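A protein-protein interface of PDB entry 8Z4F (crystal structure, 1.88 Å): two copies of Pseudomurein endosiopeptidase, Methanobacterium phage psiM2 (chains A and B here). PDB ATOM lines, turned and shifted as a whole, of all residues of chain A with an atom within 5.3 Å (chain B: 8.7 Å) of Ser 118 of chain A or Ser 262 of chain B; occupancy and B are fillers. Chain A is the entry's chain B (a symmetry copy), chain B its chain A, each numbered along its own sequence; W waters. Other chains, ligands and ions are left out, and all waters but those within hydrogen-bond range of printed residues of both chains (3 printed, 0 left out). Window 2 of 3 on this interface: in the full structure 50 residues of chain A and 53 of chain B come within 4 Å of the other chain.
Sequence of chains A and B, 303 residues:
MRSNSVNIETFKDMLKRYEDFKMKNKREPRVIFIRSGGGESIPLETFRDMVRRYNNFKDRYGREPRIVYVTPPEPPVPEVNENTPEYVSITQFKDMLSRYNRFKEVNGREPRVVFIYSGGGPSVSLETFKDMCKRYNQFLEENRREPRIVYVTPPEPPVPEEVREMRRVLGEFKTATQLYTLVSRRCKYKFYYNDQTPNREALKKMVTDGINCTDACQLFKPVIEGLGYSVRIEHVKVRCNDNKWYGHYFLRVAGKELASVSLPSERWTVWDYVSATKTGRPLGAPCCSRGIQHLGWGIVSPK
Of the 15 printed residues of chain B, 8 touch a printed residue of chain A. Hydrophobic or aromatic side chains of chain B within 4 Å of the printed part of chain A: Val 261 and Trp 268. Of the 8 printed residues of chain A, 4 touch a printed residue of chain B. Hydrophobic or aromatic side chains of chain A within 4 Å of the printed part of chain B: Tyr 117. Among the printed residues, 10 pairs touch across the chains.
Arg 99 of chain A touches none of the printed residues of chain B. Of the printed residues of chain B, Tyr 117 of chain A touches Arg 232 (3.5 Å), Ser 265 (3.9 Å) and Trp 268 (3.8 Å). Ser 118 of chain A touches three residues of chain B. No residue of chain B comes within 4 Å of Gly 119 of chain A. Printed residues of chain A within 4 Å of Ser 230 of chain B: Gln 92. Ser 260 of chain B touches none of the printed residues of chain A. Of chain A, only Asp 95 (3.6 Å) and Ser 118 (2.7 Å) come within 4 Å of Ser 262 of chain B. Of the printed residues of chain A, Pro 264 of chain B touches Ser 118. Of the printed residues of chain A, Trp 268 of chain B touches Gln 92 (3.2 Å) and Tyr 117 (3.8 Å). The nearest printed residue of chain A that does not touch Val 261 of chain B is Asp 95 of chain A (4.1 Å).
O of Ala 254 of chain B is in hydrogen-bond range of N of Ser 230 of chain B, 2.9 Å away. The side-chain hydroxyl of Ser 260 of chain B lies within hydrogen-bond range of the side-chain hydroxyl of Ser 262 of chain B (3.0 Å). The backbone carbonyl oxygen (O) of Val 261 of chain B sits at hydrogen-bond distance from the indole nitrogen (NE1) of Trp 268 of chain B (3.5 Å). The backbone carbonyl oxygen of Leu 263 of chain B sits at hydrogen-bond distance from the indole nitrogen of Trp 268 of chain B (2.9 Å). The backbone carbonyl oxygen (O) of Ile 116 of chain A lies within hydrogen-bond range of the side-chain amide nitrogen (NE2) of Gln 92 of chain A. The side-chain carboxylate (OD2) of Asp 95 of chain A is in salt-bridge range of the guanidinium group (NE) of Arg 99 of chain A, 2.9 Å away.
No position is printed for both chains.
OE1 of Gln 92 of chain A lies within hydrogen-bond range of OG of Ser 230 of chain B (2.6 Å). The backbone carbonyl oxygen (O) of Ser 262 of chain B sits at hydrogen-bond distance from the side-chain hydroxyl (OG) of Ser 118 of chain A (2.7 Å).
Water W3 lies within hydrogen-bond range of the backbone carbonyl oxygen (O) of Gly 120 of chain A (2.7 Å), the guanidinium group (NH1) of Arg 232 of chain B (3.0 Å) and the backbone carbonyl oxygen (O) of Ser 118 of chain A (3.0 Å). Water W2 lies within hydrogen-bond range of the side-chain hydroxyl (OG) of Ser 265 of chain B (2.7 Å), the backbone carbonyl oxygen (O) of Leu 263 of chain B (2.8 Å) and the backbone carbonyl oxygen (O) of Ser 118 of chain A (2.8 Å). Water W1 lies within hydrogen-bond range of the backbone carbonyl oxygen (O) of Val 261 of chain B (2.7 Å), the backbone NH (N) of Ser 118 of chain A (2.8 Å), the side-chain amide nitrogen (NE2) of Gln 92 of chain A (2.9 Å) and the side-chain carboxylate (OD2) of Asp 95 of chain A (3.0 Å).
OE1 of Gln 92 of chain A touches CG2 of Val 261 of chain B (3.4 Å). Gln 92 of chain A touches Trp 268 of chain B. Ser 262 of chain B touches Asp 95 of chain A. Tyr 117 of chain A touches Arg 232 of chain B. Tyr 117 of chain A touches Ser 265 of chain B (CB to OG, 3.9 Å). Trp 268 of chain B touches Tyr 117 of chain A (CH2 to CD1, 3.8 Å). C of Leu 263 of chain B touches OG of Ser 118 of chain A, at 3.6 Å. O of Ser 118 of chain A touches CA of Pro 264 of chain B (3.5 Å).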
ATOM      1  N   GLN A  92       5.012  23.838  20.574  1.00  0.00           N
ATOM      2  CA  GLN A  92       4.084  24.197  19.504  1.00  0.00           C
ATOM      3  C   GLN A  92       4.768  24.137  18.145  1.00  0.00           C
ATOM      4  O   GLN A  92       4.183  23.673  17.160  1.00  0.00           O
ATOM      5  CB  GLN A  92       3.534  25.605  19.766  1.00  0.00           C
ATOM      6  CG  GLN A  92       2.197  25.875  19.027  1.00  0.00           C
ATOM      7  CD  GLN A  92       1.145  24.844  19.413  1.00  0.00           C
ATOM      8  OE1 GLN A  92       0.866  24.665  20.585  1.00  0.00           O
ATOM      9  NE2 GLN A  92       0.556  24.150  18.418  1.00  0.00           N
ATOM     10  N   ASP A  95       4.917  20.675  17.007  1.00  0.00           N
ATOM     11  CA  ASP A  95       3.599  20.226  16.550  1.00  0.00           C
ATOM     12  C   ASP A  95       3.289  20.762  15.146  1.00  0.00           C
ATOM     13  O   ASP A  95       2.681  20.062  14.317  1.00  0.00           O
ATOM     14  CB  ASP A  95       2.519  20.666  17.538  1.00  0.00           C
ATOM     15  CG  ASP A  95       1.151  20.108  17.169  1.00  0.00           C
ATOM     16  OD1 ASP A  95       0.975  18.899  17.347  1.00  0.00           O
ATOM     17  OD2 ASP A  95       0.272  20.881  16.710  1.00  0.00           O
ATOM     18  N   ARG A  99       2.437  18.509  11.778  1.00  0.00           N
ATOM     19  CA  ARG A  99       1.283  18.758  10.871  1.00  0.00           C
ATOM     20  C   ARG A  99       1.805  19.117   9.468  1.00  0.00           C
ATOM     21  O   ARG A  99       1.184  18.728   8.498  1.00  0.00           O
ATOM     22  CB  ARG A  99       0.266  19.727  11.481  1.00  0.00           C
ATOM     23  CG  ARG A  99      -0.649  19.079  12.511  1.00  0.00           C
ATOM     24  CD  ARG A  99      -1.649  19.988  13.188  1.00  0.00           C
ATOM     25  NE  ARG A  99      -0.932  20.918  14.019  1.00  0.00           N
ATOM     26  CZ  ARG A  99      -0.639  22.156  13.695  1.00  0.00           C
ATOM     27  NH1 ARG A  99      -1.035  22.657  12.545  1.00  0.00           N
ATOM     28  NH2 ARG A  99       0.056  22.895  14.523  1.00  0.00           N
ATOM     29  N   ILE A 116      -0.974  27.347  13.364  1.00  0.00           N
ATOM     30  CA  ILE A 116      -0.116  27.339  14.555  1.00  0.00           C
ATOM     31  C   ILE A 116      -0.535  26.223  15.502  1.00  0.00           C
ATOM     32  O   ILE A 116       0.313  25.458  15.994  1.00  0.00           O
ATOM     33  CB  ILE A 116      -0.136  28.715  15.237  1.00  0.00           C
ATOM     34  CG1 ILE A 116       0.660  29.692  14.360  1.00  0.00           C
ATOM     35  CG2 ILE A 116       0.477  28.626  16.644  1.00  0.00           C
ATOM     36  CD1 ILE A 116       0.672  31.080  14.846  1.00  0.00           C
ATOM     37  N   TYR A 117      -1.844  26.066  15.708  1.00  0.00           N
ATOM     38  CA  TYR A 117      -2.412  25.104  16.644  1.00  0.00           C
ATOM     39  C   TYR A 117      -3.236  24.051  15.913  1.00  0.00           C
ATOM     40  O   TYR A 117      -3.969  24.352  14.974  1.00  0.00           O
ATOM     41  CB  TYR A 117      -3.331  25.780  17.664  1.00  0.00           C
ATOM     42  CG  TYR A 117      -2.681  26.978  18.365  1.00  0.00           C
ATOM     43  CD1 TYR A 117      -1.771  26.788  19.399  1.00  0.00           C
ATOM     44  CD2 TYR A 117      -2.987  28.280  17.990  1.00  0.00           C
ATOM     45  CE1 TYR A 117      -1.173  27.875  20.054  1.00  0.00           C
ATOM     46  CE2 TYR A 117      -2.383  29.369  18.632  1.00  0.00           C
ATOM     47  CZ  TYR A 117      -1.497  29.161  19.663  1.00  0.00           C
ATOM     48  OH  TYR A 117      -0.928  30.259  20.298  1.00  0.00           O
ATOM     49  N   SER A 118      -3.171  22.841  16.417  1.00  0.00           N
ATOM     50  CA  SER A 118      -4.117  21.808  16.019  1.00  0.00           C
ATOM     51  C   SER A 118      -5.550  22.290  16.237  1.00  0.00           C
ATOM     52  O   SER A 118      -5.874  22.892  17.265  1.00  0.00           O
ATOM     53  CB  SER A 118      -3.823  20.546  16.820  1.00  0.00           C
ATOM     54  OG  SER A 118      -4.966  19.751  17.007  1.00  0.00           O
ATOM     55  N   GLY A 119      -6.398  22.090  15.228  1.00  0.00           N
ATOM     56  CA  GLY A 119      -7.795  22.500  15.290  1.00  0.00           C
ATOM     57  C   GLY A 119      -8.106  23.775  14.535  1.00  0.00           C
ATOM     58  O   GLY A 119      -9.281  24.125  14.421  1.00  0.00           O
ATOM     59  N   GLY A 120      -7.098  24.485  14.030  1.00  0.00           N
ATOM     60  CA  GLY A 120      -7.329  25.700  13.264  1.00  0.00           C
ATOM     61  C   GLY A 120      -7.057  26.967  14.059  1.00  0.00           C
ATOM     62  O   GLY A 120      -6.541  26.946  15.174  1.00  0.00           O
ATOM     63  N   SER B 230       3.302  25.005  25.654  1.00  0.00           N
ATOM     64  CA  SER B 230       2.538  25.922  24.825  1.00  0.00           C
ATOM     65  C   SER B 230       1.379  26.462  25.665  1.00  0.00           C
ATOM     66  O   SER B 230       0.801  25.741  26.475  1.00  0.00           O
ATOM     67  CB  SER B 230       2.034  25.221  23.542  1.00  0.00           C
ATOM     68  OG  SER B 230       1.535  26.196  22.628  1.00  0.00           O
ATOM     69  N   ARG B 232      -2.211  29.094  25.516  1.00  0.00           N
ATOM     70  CA  ARG B 232      -3.214  29.918  24.805  1.00  0.00           C
ATOM     71  C   ARG B 232      -4.204  30.466  25.843  1.00  0.00           C
ATOM     72  O   ARG B 232      -4.702  29.688  26.616  1.00  0.00           O
ATOM     73  CB  ARG B 232      -3.926  29.045  23.777  1.00  0.00           C
ATOM     74  CG  ARG B 232      -3.995  29.630  22.386  1.00  0.00           C
ATOM     75  CD  ARG B 232      -4.653  28.666  21.442  1.00  0.00           C
ATOM     76  NE  ARG B 232      -5.399  29.366  20.433  1.00  0.00           N
ATOM     77  CZ  ARG B 232      -6.119  28.744  19.529  1.00  0.00           C
ATOM     78  NH1 ARG B 232      -6.153  27.429  19.517  1.00  0.00           N
ATOM     79  NH2 ARG B 232      -6.792  29.431  18.639  1.00  0.00           N
ATOM     80  N   ALA B 254      -0.359  23.078  27.363  1.00  0.00           N
ATOM     81  CA  ALA B 254      -0.019  21.770  26.809  1.00  0.00           C
ATOM     82  C   ALA B 254       1.493  21.602  26.846  1.00  0.00           C
ATOM     83  O   ALA B 254       2.235  22.591  26.885  1.00  0.00           O
ATOM     84  CB  ALA B 254      -0.525  21.614  25.356  1.00  0.00           C
ATOM     85  N   GLY B 255       1.942  20.349  26.831  1.00  0.00           N
ATOM     86  CA  GLY B 255       3.355  19.987  26.797  1.00  0.00           C
ATOM     87  C   GLY B 255       3.819  19.354  28.114  1.00  0.00           C
ATOM     88  O   GLY B 255       3.168  19.463  29.161  1.00  0.00           O
ATOM     89  N   ALA B 259      -1.273  18.581  29.092  1.00  0.00           N
ATOM     90  CA  ALA B 259      -2.041  17.982  27.997  1.00  0.00           C
ATOM     91  C   ALA B 259      -1.206  17.801  26.733  1.00  0.00           C
ATOM     92  O   ALA B 259      -0.262  18.555  26.460  1.00  0.00           O
ATOM     93  CB  ALA B 259      -3.245  18.853  27.668  1.00  0.00           C
ATOM     94  N   SER B 260      -1.580  16.789  25.933  1.00  0.00           N
ATOM     95  CA  SER B 260      -0.930  16.576  24.643  1.00  0.00           C
ATOM     96  C   SER B 260      -1.178  17.784  23.747  1.00  0.00           C
ATOM     97  O   SER B 260      -2.325  18.224  23.569  1.00  0.00           O
ATOM     98  CB  SER B 260      -1.476  15.307  23.973  1.00  0.00           C
ATOM     99  OG  SER B 260      -1.001  15.198  22.640  1.00  0.00           O
ATOM    100  N   VAL B 261      -0.098  18.320  23.184  1.00  0.00           N
ATOM    101  CA  VAL B 261      -0.187  19.527  22.366  1.00  0.00           C
ATOM    102  C   VAL B 261      -0.981  19.288  21.072  1.00  0.00           C
ATOM    103  O   VAL B 261      -1.567  20.226  20.504  1.00  0.00           O
ATOM    104  CB  VAL B 261       1.237  20.032  22.080  1.00  0.00           C
ATOM    105  CG1 VAL B 261       2.033  19.012  21.266  1.00  0.00           C
ATOM    106  CG2 VAL B 261       1.202  21.401  21.397  1.00  0.00           C
ATOM    107  N   SER B 262      -1.008  18.052  20.579  1.00  0.00           N
ATOM    108  CA  SER B 262      -1.756  17.759  19.353  1.00  0.00           C
ATOM    109  C   SER B 262      -3.270  17.772  19.551  1.00  0.00           C
ATOM    110  O   SER B 262      -4.022  17.774  18.556  1.00  0.00           O
ATOM    111  CB  SER B 262      -1.238  16.446  18.752  1.00  0.00           C
ATOM    112  OG  SER B 262      -1.340  15.329  19.629  1.00  0.00           O
ATOM    113  N   LEU B 263      -3.744  17.826  20.797  1.00  0.00           N
ATOM    114  CA  LEU B 263      -5.160  18.061  21.038  1.00  0.00           C
ATOM    115  C   LEU B 263      -5.516  19.480  20.604  1.00  0.00           C
ATOM    116  O   LEU B 263      -4.682  20.378  20.705  1.00  0.00           O
ATOM    117  CB  LEU B 263      -5.451  17.915  22.523  1.00  0.00           C
ATOM    118  CG  LEU B 263      -5.558  16.476  23.010  1.00  0.00           C
ATOM    119  CD1 LEU B 263      -5.548  16.503  24.552  1.00  0.00           C
ATOM    120  CD2 LEU B 263      -6.824  15.766  22.486  1.00  0.00           C
ATOM    121  N   PRO B 264      -6.743  19.711  20.130  1.00  0.00           N
ATOM    122  CA  PRO B 264      -7.219  21.089  19.983  1.00  0.00           C
ATOM    123  C   PRO B 264      -7.145  21.817  21.319  1.00  0.00           C
ATOM    124  O   PRO B 264      -7.371  21.232  22.384  1.00  0.00           O
ATOM    125  CB  PRO B 264      -8.671  20.931  19.512  1.00  0.00           C
ATOM    126  CG  PRO B 264      -8.984  19.479  19.626  1.00  0.00           C
ATOM    127  CD  PRO B 264      -7.745  18.708  19.721  1.00  0.00           C
ATOM    128  N   SER B 265      -6.839  23.118  21.253  1.00  0.00           N
ATOM    129  CA  SER B 265      -6.442  23.833  22.472  1.00  0.00           C
ATOM    130  C   SER B 265      -7.559  23.864  23.504  1.00  0.00           C
ATOM    131  O   SER B 265      -7.286  23.966  24.702  1.00  0.00           O
ATOM    132  CB  SER B 265      -5.993  25.257  22.128  1.00  0.00           C
ATOM    133  OG  SER B 265      -4.907  25.198  21.218  1.00  0.00           O
ATOM    134  N   GLU B 266      -8.819  23.735  23.081  1.00  0.00           N
ATOM    135  CA  GLU B 266      -9.869  23.765  24.082  1.00  0.00           C
ATOM    136  C   GLU B 266      -9.971  22.454  24.848  1.00  0.00           C
ATOM    137  O   GLU B 266     -10.819  22.354  25.725  1.00  0.00           O
ATOM    138  CB  GLU B 266     -11.209  24.131  23.448  1.00  0.00           C
ATOM    139  CG  GLU B 266     -11.702  23.093  22.453  1.00  0.00           C
ATOM    140  CD  GLU B 266     -11.336  23.446  21.005  1.00  0.00           C
ATOM    141  OE1 GLU B 266     -10.255  24.036  20.774  1.00  0.00           O
ATOM    142  OE2 GLU B 266     -12.113  23.086  20.084  1.00  0.00           O
ATOM    143  N   ARG B 267      -9.110  21.472  24.568  1.00  0.00           N
ATOM    144  CA  ARG B 267      -8.957  20.278  25.395  1.00  0.00           C
ATOM    145  C   ARG B 267      -7.655  20.288  26.201  1.00  0.00           C
ATOM    146  O   ARG B 267      -7.261  19.240  26.747  1.00  0.00           O
ATOM    147  CB  ARG B 267      -8.957  19.023  24.524  1.00  0.00           C
ATOM    148  CG  ARG B 267     -10.182  18.839  23.645  1.00  0.00           C
ATOM    149  CD  ARG B 267     -11.435  18.500  24.386  1.00  0.00           C
ATOM    150  NE  ARG B 267     -12.399  17.907  23.460  1.00  0.00           N
ATOM    151  CZ  ARG B 267     -13.550  17.373  23.830  1.00  0.00           C
ATOM    152  NH1 ARG B 267     -13.884  17.275  25.107  1.00  0.00           N
ATOM    153  NH2 ARG B 267     -14.385  16.922  22.895  1.00  0.00           N
ATOM    154  N   TRP B 268      -6.919  21.392  26.158  1.00  0.00           N
ATOM    155  CA  TRP B 268      -5.643  21.439  26.908  1.00  0.00           C
ATOM    156  C   TRP B 268      -5.917  21.567  28.420  1.00  0.00           C
ATOM    157  O   TRP B 268      -7.021  21.847  28.846  1.00  0.00           O
ATOM    158  CB  TRP B 268      -4.745  22.577  26.393  1.00  0.00           C
ATOM    159  CG  TRP B 268      -4.123  22.424  25.036  1.00  0.00           C
ATOM    160  CD1 TRP B 268      -4.206  21.365  24.187  1.00  0.00           C
ATOM    161  CD2 TRP B 268      -3.292  23.383  24.366  1.00  0.00           C
ATOM    162  NE1 TRP B 268      -3.493  21.599  23.048  1.00  0.00           N
ATOM    163  CE2 TRP B 268      -2.925  22.833  23.127  1.00  0.00           C
ATOM    164  CE3 TRP B 268      -2.825  24.657  24.693  1.00  0.00           C
ATOM    165  CZ2 TRP B 268      -2.120  23.514  22.223  1.00  0.00           C
ATOM    166  CZ3 TRP B 268      -2.020  25.323  23.805  1.00  0.00           C
ATOM    167  CH2 TRP B 268      -1.674  24.760  22.584  1.00  0.00           C
ATOM    168  N   TRP B 297     -10.429  33.400  21.992  1.00  0.00           N
ATOM    169  CA  TRP B 297      -9.028  33.225  22.356  1.00  0.00           C
ATOM    170  C   TRP B 297      -8.361  34.590  22.440  1.00  0.00           C
ATOM    171  O   TRP B 297      -8.485  35.402  21.519  1.00  0.00           O
ATOM    172  CB  TRP B 297      -8.283  32.344  21.346  1.00  0.00           C
ATOM    173  CG  TRP B 297      -8.766  30.927  21.281  1.00  0.00           C
ATOM    174  CD1 TRP B 297      -9.551  30.373  20.305  1.00  0.00           C
ATOM    175  CD2 TRP B 297      -8.510  29.878  22.234  1.00  0.00           C
ATOM    176  NE1 TRP B 297      -9.786  29.047  20.585  1.00  0.00           N
ATOM    177  CE2 TRP B 297      -9.168  28.719  21.764  1.00  0.00           C
ATOM    178  CE3 TRP B 297      -7.794  29.808  23.438  1.00  0.00           C
ATOM    179  CZ2 TRP B 297      -9.128  27.495  22.454  1.00  0.00           C
ATOM    180  CZ3 TRP B 297      -7.754  28.601  24.117  1.00  0.00           C
ATOM    181  CH2 TRP B 297      -8.427  27.457  23.628  1.00  0.00           C
HETATM  182  O   HOH W   1      -1.606  22.218  18.626  1.00  0.00           O
HETATM  183  O   HOH W   2      -4.484  22.999  19.726  1.00  0.00           O
HETATM  184  O   HOH W   3      -7.162  25.602  17.385  1.00  0.00           O
